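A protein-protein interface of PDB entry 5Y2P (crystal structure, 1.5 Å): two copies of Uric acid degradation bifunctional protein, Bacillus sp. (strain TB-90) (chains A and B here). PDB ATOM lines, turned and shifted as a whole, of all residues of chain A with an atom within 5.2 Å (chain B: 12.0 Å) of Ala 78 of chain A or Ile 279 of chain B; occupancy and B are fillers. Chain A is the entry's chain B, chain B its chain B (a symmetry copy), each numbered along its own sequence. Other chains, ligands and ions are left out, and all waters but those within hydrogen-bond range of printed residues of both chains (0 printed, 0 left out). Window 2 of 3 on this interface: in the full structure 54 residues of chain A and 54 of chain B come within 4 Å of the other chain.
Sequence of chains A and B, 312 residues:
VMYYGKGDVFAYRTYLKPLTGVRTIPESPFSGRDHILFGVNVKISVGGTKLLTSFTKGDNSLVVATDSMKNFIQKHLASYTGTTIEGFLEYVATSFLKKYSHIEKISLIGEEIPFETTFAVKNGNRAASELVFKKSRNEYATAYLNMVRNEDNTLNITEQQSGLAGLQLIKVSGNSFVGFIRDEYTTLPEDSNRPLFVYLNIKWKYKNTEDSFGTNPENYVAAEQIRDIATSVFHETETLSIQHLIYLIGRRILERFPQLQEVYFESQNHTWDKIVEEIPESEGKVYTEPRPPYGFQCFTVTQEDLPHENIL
NE of Arg 13 of chain A touches CD1 of Ile 279 of chain B, 3.7 Å away. Lys 285 of chain B touches Arg 13 of chain A. CA of Gly 284 of chain B touches O of Thr 14 of chain A, 3.2 Å away. Gln 74 of chain A touches Ile 275 of chain B. Gln 74 of chain A touches Val 286 of chain B (O to CG1, 3.9 Å). Ala 78 of chain A touches Val 276 of chain B (CB to CG2, 3.8 Å). CG2 of Ile 279 of chain B touches O of Ala 78 of chain A, 3.3 Å away. Ala 78 of chain A touches Val 286 of chain B.
The side-chain hydroxyl (OG1) of Thr 14 of chain A lies within hydrogen-bond range of the backbone NH (N) of Lys 285 of chain B. The side-chain amide nitrogen (NE2) of Gln 74 of chain A is in hydrogen-bond range of the side-chain hydroxyl (OG1) of Thr 288 of chain B, 3.1 Å away.
No position is printed for both chains.
The guanidinium group of Arg 13 of chain A lies within hydrogen-bond range of the backbone carbonyl oxygen of Leu 77 of chain A. NH1 of Arg 13 of chain A is in hydrogen-bond range of O of Ala 78 of chain A (3.3 Å). The guanidinium group (NH1) of Arg 13 of chain A sits at hydrogen-bond distance from the backbone carbonyl oxygen (O) of Tyr 80 of chain A. N of Thr 288 of chain B is in hydrogen-bond range of O of Asp 273 of chain B (2.8 Å). The backbone NH (N) of Ile 275 of chain B lies within hydrogen-bond range of the backbone carbonyl oxygen (O) of Val 286 of chain B, 2.8 Å away. The backbone NH (N) of Val 276 of chain B is in hydrogen-bond range of the backbone carbonyl oxygen (O) of Val 286 of chain B, 3.1 Å away.
Printed residues of chain B within 4 Å of Gln 74 of chain A: Ile 275, Val 286 and Thr 288. No residue of chain B comes within 4 Å of Leu 77 of chain A. Printed residues of chain B within 4 Å of Ala 78 of chain A: Val 276, Ile 279 and Val 286. Lys 274 of chain B touches none of the printed residues of chain A. Of the printed residues of chain A, Ile 275 of chain B touches Gln 74 (3.8 Å). Ile 279 of chain B touches just these residues of chain A: Arg 13 and Ala 78. Printed residues of chain A within 4 Å of Gly 284 of chain B: Thr 14 (3.2 Å). Printed residues of chain A within 4 Å of Val 286 of chain B: Gln 74 (3.9 Å) and Ala 78 (3.6 Å). Printed residues of chain A within 4 Å of Thr 288 of chain B: Gln 74. The nearest printed residue of chain B that does not touch Ala 78 of chain A is Lys 285 of chain B (5.9 Å).
Of the 16 printed residues of chain B, 7 touch a printed residue of chain A. Printed residues of chain B that touch a printed residue of chain A: Ile 275, Val 276, Ile 279, Gly 284, Lys 285, Val 286 and Thr 288. Hydrophobic or aromatic side chains of chain B within 4 Å of the printed part of chain A: Ile 275, Val 276, Ile 279 and Val 286. Hydrophobic or aromatic side chains of chain A within 4 Å of the printed part of chain B: Ala 78. Along chain A the printed residues that touch a printed residue of chain B span positions 13 to 78. Among the printed residues, 10 pairs touch across the chains. Among the printed residues, no Asp or Glu carboxylate lies within 4 Å of a Lys or Arg side-chain nitrogen of the other chain.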
ATOM      1  N   ARG A  13       8.615  -2.010  33.584  1.00  0.00           N
ATOM      2  CA  ARG A  13       7.695  -2.626  32.636  1.00  0.00           C
ATOM      3  C   ARG A  13       6.604  -3.340  33.424  1.00  0.00           C
ATOM      4  O   ARG A  13       6.903  -4.058  34.374  1.00  0.00           O
ATOM      5  CB  ARG A  13       8.498  -3.634  31.791  1.00  0.00           C
ATOM      6  CG  ARG A  13       7.717  -4.665  30.965  1.00  0.00           C
ATOM      7  CD  ARG A  13       7.083  -4.107  29.699  1.00  0.00           C
ATOM      8  NE  ARG A  13       6.224  -5.157  29.144  1.00  0.00           N
ATOM      9  CZ  ARG A  13       6.527  -5.974  28.138  1.00  0.00           C
ATOM     10  NH1 ARG A  13       7.668  -5.903  27.473  1.00  0.00           N
ATOM     11  NH2 ARG A  13       5.653  -6.928  27.820  1.00  0.00           N
ATOM     12  N   THR A  14       5.355  -3.151  33.037  1.00  0.00           N
ATOM     13  CA  THR A  14       4.266  -3.925  33.606  1.00  0.00           C
ATOM     14  C   THR A  14       3.950  -5.082  32.671  1.00  0.00           C
ATOM     15  O   THR A  14       4.112  -4.973  31.450  1.00  0.00           O
ATOM     16  CB  THR A  14       3.027  -3.089  33.919  1.00  0.00           C
ATOM     17  OG1 THR A  14       2.614  -2.382  32.743  1.00  0.00           O
ATOM     18  CG2 THR A  14       3.285  -2.079  35.060  1.00  0.00           C
ATOM     19  N   GLN A  74      14.992   1.894  26.769  1.00  0.00           N
ATOM     20  CA  GLN A  74      13.630   1.962  27.288  1.00  0.00           C
ATOM     21  C   GLN A  74      12.619   1.461  26.263  1.00  0.00           C
ATOM     22  O   GLN A  74      11.689   0.714  26.619  1.00  0.00           O
ATOM     23  CB  GLN A  74      13.336   3.392  27.766  1.00  0.00           C
ATOM     24  CG  GLN A  74      14.222   3.745  28.967  1.00  0.00           C
ATOM     25  CD  GLN A  74      14.055   5.176  29.449  1.00  0.00           C
ATOM     26  OE1 GLN A  74      13.602   6.053  28.718  1.00  0.00           O
ATOM     27  NE2 GLN A  74      14.464   5.423  30.696  1.00  0.00           N
ATOM     28  N   LYS A  75      12.808   1.804  24.979  1.00  0.00           N
ATOM     29  CA  LYS A  75      11.935   1.302  23.915  1.00  0.00           C
ATOM     30  C   LYS A  75      12.044  -0.208  23.769  1.00  0.00           C
ATOM     31  O   LYS A  75      11.038  -0.892  23.530  1.00  0.00           O
ATOM     32  CB  LYS A  75      12.277   1.963  22.587  1.00  0.00           C
ATOM     33  CG  LYS A  75      11.787   3.378  22.467  1.00  0.00           C
ATOM     34  CD  LYS A  75      12.321   3.954  21.158  1.00  0.00           C
ATOM     35  CE  LYS A  75      11.464   5.067  20.589  1.00  0.00           C
ATOM     36  NZ  LYS A  75      12.037   5.489  19.275  1.00  0.00           N
ATOM     37  N   HIS A  76      13.250  -0.754  23.946  1.00  0.00           N
ATOM     38  CA  HIS A  76      13.411  -2.196  23.803  1.00  0.00           C
ATOM     39  C   HIS A  76      12.820  -2.953  24.980  1.00  0.00           C
ATOM     40  O   HIS A  76      12.400  -4.106  24.806  1.00  0.00           O
ATOM     41  CB  HIS A  76      14.867  -2.565  23.525  1.00  0.00           C
ATOM     42  CG  HIS A  76      15.236  -2.376  22.094  1.00  0.00           C
ATOM     43  ND1 HIS A  76      15.417  -1.124  21.545  1.00  0.00           N
ATOM     44  CD2 HIS A  76      15.387  -3.260  21.081  1.00  0.00           C
ATOM     45  CE1 HIS A  76      15.694  -1.248  20.257  1.00  0.00           C
ATOM     46  NE2 HIS A  76      15.665  -2.532  19.942  1.00  0.00           N
ATOM     47  N   LEU A  77      12.740  -2.339  26.164  1.00  0.00           N
ATOM     48  CA  LEU A  77      12.027  -3.027  27.237  1.00  0.00           C
ATOM     49  C   LEU A  77      10.552  -3.163  26.893  1.00  0.00           C
ATOM     50  O   LEU A  77       9.910  -4.168  27.245  1.00  0.00           O
ATOM     51  CB  LEU A  77      12.248  -2.360  28.603  1.00  0.00           C
ATOM     52  CG  LEU A  77      11.603  -3.131  29.766  1.00  0.00           C
ATOM     53  CD1 LEU A  77      12.174  -4.550  29.873  1.00  0.00           C
ATOM     54  CD2 LEU A  77      11.817  -2.355  31.071  1.00  0.00           C
ATOM     55  N   ALA A  78       9.993  -2.202  26.165  1.00  0.00           N
ATOM     56  CA  ALA A  78       8.596  -2.285  25.752  1.00  0.00           C
ATOM     57  C   ALA A  78       8.358  -3.414  24.751  1.00  0.00           C
ATOM     58  O   ALA A  78       7.296  -4.044  24.766  1.00  0.00           O
ATOM     59  CB  ALA A  78       8.129  -0.950  25.155  1.00  0.00           C
ATOM     60  N   SER A  79       9.311  -3.662  23.846  1.00  0.00           N
ATOM     61  CA  SER A  79       9.129  -4.660  22.803  1.00  0.00           C
ATOM     62  C   SER A  79       9.693  -6.028  23.175  1.00  0.00           C
ATOM     63  O   SER A  79       9.541  -6.971  22.391  1.00  0.00           O
ATOM     64  CB  SER A  79       9.766  -4.178  21.486  1.00  0.00           C
ATOM     65  OG  SER A  79      11.100  -3.850  21.665  1.00  0.00           O
ATOM     66  N   TYR A  80      10.297  -6.167  24.355  1.00  0.00           N
ATOM     67  CA  TYR A  80      10.913  -7.430  24.759  1.00  0.00           C
ATOM     68  C   TYR A  80       9.843  -8.464  25.083  1.00  0.00           C
ATOM     69  O   TYR A  80       8.974  -8.225  25.920  1.00  0.00           O
ATOM     70  CB  TYR A  80      11.811  -7.196  25.990  1.00  0.00           C
ATOM     71  CG  TYR A  80      12.494  -8.453  26.511  1.00  0.00           C
ATOM     72  CD1 TYR A  80      13.222  -9.263  25.669  1.00  0.00           C
ATOM     73  CD2 TYR A  80      12.378  -8.820  27.838  1.00  0.00           C
ATOM     74  CE1 TYR A  80      13.811 -10.410  26.125  1.00  0.00           C
ATOM     75  CE2 TYR A  80      13.002  -9.983  28.318  1.00  0.00           C
ATOM     76  CZ  TYR A  80      13.690 -10.772  27.442  1.00  0.00           C
ATOM     77  OH  TYR A  80      14.296 -11.951  27.878  1.00  0.00           O
ATOM     78  N   ASP B 273       7.629   8.566  35.507  1.00  0.00           N
ATOM     79  CA  ASP B 273       7.221   9.170  34.247  1.00  0.00           C
ATOM     80  C   ASP B 273       6.974   8.088  33.202  1.00  0.00           C
ATOM     81  O   ASP B 273       7.737   7.127  33.091  1.00  0.00           O
ATOM     82  CB  ASP B 273       8.345  10.087  33.729  1.00  0.00           C
ATOM     83  CG  ASP B 273       8.425  11.424  34.465  1.00  0.00           C
ATOM     84  OD1 ASP B 273       7.407  11.856  35.038  1.00  0.00           O
ATOM     85  OD2 ASP B 273       9.510  12.067  34.447  1.00  0.00           O
ATOM     86  N   LYS B 274       5.930   8.258  32.405  1.00  0.00           N
ATOM     87  CA  LYS B 274       5.618   7.294  31.360  1.00  0.00           C
ATOM     88  C   LYS B 274       6.486   7.500  30.126  1.00  0.00           C
ATOM     89  O   LYS B 274       6.692   8.628  29.667  1.00  0.00           O
ATOM     90  CB  LYS B 274       4.134   7.370  30.985  1.00  0.00           C
ATOM     91  CG  LYS B 274       3.671   6.194  30.118  1.00  0.00           C
ATOM     92  CD  LYS B 274       2.218   6.380  29.694  1.00  0.00           C
ATOM     93  CE  LYS B 274       1.290   6.356  30.893  1.00  0.00           C
ATOM     94  N   ILE B 275       6.929   6.384  29.551  1.00  0.00           N
ATOM     95  CA  ILE B 275       7.712   6.350  28.323  1.00  0.00           C
ATOM     96  C   ILE B 275       6.907   5.744  27.186  1.00  0.00           C
ATOM     97  O   ILE B 275       6.864   6.294  26.093  1.00  0.00           O
ATOM     98  CB  ILE B 275       9.031   5.561  28.524  1.00  0.00           C
ATOM     99  CG1 ILE B 275       9.894   6.159  29.628  1.00  0.00           C
ATOM    100  CG2 ILE B 275       9.812   5.482  27.228  1.00  0.00           C
ATOM    101  CD1 ILE B 275      10.095   7.674  29.502  1.00  0.00           C
ATOM    102  N   VAL B 276       6.295   4.580  27.419  1.00  0.00           N
ATOM    103  CA  VAL B 276       5.528   3.864  26.401  1.00  0.00           C
ATOM    104  C   VAL B 276       4.137   3.609  26.960  1.00  0.00           C
ATOM    105  O   VAL B 276       3.999   2.974  28.013  1.00  0.00           O
ATOM    106  CB  VAL B 276       6.184   2.528  25.994  1.00  0.00           C
ATOM    107  CG1 VAL B 276       5.315   1.793  24.959  1.00  0.00           C
ATOM    108  CG2 VAL B 276       7.592   2.757  25.454  1.00  0.00           C
ATOM    109  N   GLU B 277       3.108   4.067  26.235  1.00  0.00           N
ATOM    110  CA  GLU B 277       1.726   3.964  26.696  1.00  0.00           C
ATOM    111  C   GLU B 277       1.027   2.714  26.181  1.00  0.00           C
ATOM    112  O   GLU B 277       0.110   2.208  26.841  1.00  0.00           O
ATOM    113  CB  GLU B 277       0.922   5.195  26.251  1.00  0.00           C
ATOM    114  N   GLU B 278       1.432   2.205  25.020  1.00  0.00           N
ATOM    115  CA  GLU B 278       0.780   1.054  24.410  1.00  0.00           C
ATOM    116  C   GLU B 278       1.846   0.100  23.893  1.00  0.00           C
ATOM    117  O   GLU B 278       2.761   0.523  23.181  1.00  0.00           O
ATOM    118  CB  GLU B 278      -0.130   1.498  23.250  1.00  0.00           C
ATOM    119  N   ILE B 279       1.728  -1.172  24.249  1.00  0.00           N
ATOM    120  CA  ILE B 279       2.616  -2.226  23.759  1.00  0.00           C
ATOM    121  C   ILE B 279       1.791  -3.185  22.913  1.00  0.00           C
ATOM    122  O   ILE B 279       0.763  -3.680  23.388  1.00  0.00           O
ATOM    123  CB  ILE B 279       3.291  -2.982  24.917  1.00  0.00           C
ATOM    124  CG1 ILE B 279       4.282  -2.063  25.625  1.00  0.00           C
ATOM    125  CG2 ILE B 279       4.009  -4.242  24.410  1.00  0.00           C
ATOM    126  CD1 ILE B 279       4.763  -2.590  26.956  1.00  0.00           C
ATOM    127  N   PRO B 280       2.205  -3.482  21.684  1.00  0.00           N
ATOM    128  CA  PRO B 280       1.473  -4.461  20.874  1.00  0.00           C
ATOM    129  C   PRO B 280       1.162  -5.733  21.654  1.00  0.00           C
ATOM    130  O   PRO B 280       2.050  -6.362  22.238  1.00  0.00           O
ATOM    131  CB  PRO B 280       2.433  -4.733  19.710  1.00  0.00           C
ATOM    132  N   GLU B 281      -0.122  -6.097  21.682  1.00  0.00           N
ATOM    133  CA  GLU B 281      -0.571  -7.396  22.182  1.00  0.00           C
ATOM    134  C   GLU B 281      -0.317  -7.584  23.675  1.00  0.00           C
ATOM    135  O   GLU B 281      -0.163  -8.715  24.147  1.00  0.00           O
ATOM    136  N   SER B 282      -0.277  -6.490  24.435  1.00  0.00           N
ATOM    137  CA  SER B 282      -0.082  -6.581  25.874  1.00  0.00           C
ATOM    138  C   SER B 282      -0.783  -5.420  26.565  1.00  0.00           C
ATOM    139  O   SER B 282      -1.032  -4.368  25.969  1.00  0.00           O
ATOM    140  N   GLU B 283      -1.108  -5.631  27.839  1.00  0.00           N
ATOM    141  CA  GLU B 283      -1.596  -4.562  28.704  1.00  0.00           C
ATOM    142  C   GLU B 283      -0.470  -3.774  29.377  1.00  0.00           C
ATOM    143  O   GLU B 283      -0.758  -2.887  30.188  1.00  0.00           O
ATOM    144  N   GLY B 284       0.812  -4.069  29.053  1.00  0.00           N
ATOM    145  CA  GLY B 284       1.927  -3.443  29.751  1.00  0.00           C
ATOM    146  C   GLY B 284       2.281  -2.100  29.173  1.00  0.00           C
ATOM    147  O   GLY B 284       1.771  -1.676  28.138  1.00  0.00           O
ATOM    148  N   LYS B 285       3.205  -1.449  29.859  1.00  0.00           N
ATOM    149  CA  LYS B 285       3.654  -0.106  29.550  1.00  0.00           C
ATOM    150  C   LYS B 285       5.073  -0.030  30.095  1.00  0.00           C
ATOM    151  O   LYS B 285       5.477  -0.902  30.871  1.00  0.00           O
ATOM    152  CB  LYS B 285       2.742   0.894  30.275  1.00  0.00           C
ATOM    153  CG  LYS B 285       1.262   0.848  29.802  1.00  0.00           C
ATOM    154  CD  LYS B 285       0.389   1.714  30.692  1.00  0.00           C
ATOM    155  N   VAL B 286       5.817   1.021  29.727  1.00  0.00           N
ATOM    156  CA  VAL B 286       7.144   1.291  30.305  1.00  0.00           C
ATOM    157  C   VAL B 286       7.220   2.680  30.937  1.00  0.00           C
ATOM    158  O   VAL B 286       6.799   3.679  30.348  1.00  0.00           O
ATOM    159  CB  VAL B 286       8.282   1.093  29.274  1.00  0.00           C
ATOM    160  CG1 VAL B 286       9.674   1.441  29.872  1.00  0.00           C
ATOM    161  CG2 VAL B 286       8.267  -0.360  28.776  1.00  0.00           C
ATOM    162  N   TYR B 287       7.852   2.747  32.102  1.00  0.00           N
ATOM    163  CA  TYR B 287       8.015   3.958  32.880  1.00  0.00           C
ATOM    164  C   TYR B 287       9.479   4.122  33.270  1.00  0.00           C
ATOM    165  O   TYR B 287      10.286   3.203  33.116  1.00  0.00           O
ATOM    166  CB  TYR B 287       7.187   3.873  34.162  1.00  0.00           C
ATOM    167  CG  TYR B 287       5.733   3.592  33.961  1.00  0.00           C
ATOM    168  CD1 TYR B 287       5.276   2.298  33.932  1.00  0.00           C
ATOM    169  CD2 TYR B 287       4.820   4.619  33.841  1.00  0.00           C
ATOM    170  CE1 TYR B 287       3.919   2.016  33.765  1.00  0.00           C
ATOM    171  CE2 TYR B 287       3.464   4.353  33.646  1.00  0.00           C
ATOM    172  CZ  TYR B 287       3.039   3.053  33.632  1.00  0.00           C
ATOM    173  OH  TYR B 287       1.713   2.743  33.475  1.00  0.00           O
ATOM    174  N   THR B 288       9.822   5.319  33.747  1.00  0.00           N
ATOM    175  CA  THR B 288      11.186   5.565  34.217  1.00  0.00           C
ATOM    176  C   THR B 288      11.171   6.550  35.375  1.00  0.00           C
ATOM    177  O   THR B 288      10.136   7.116  35.722  1.00  0.00           O
ATOM    178  CB  THR B 288      12.116   6.047  33.104  1.00  0.00           C
ATOM    179  OG1 THR B 288      13.478   5.948  33.584  1.00  0.00           O
ATOM    180  CG2 THR B 288      11.782   7.469  32.705  1.00  0.00           C
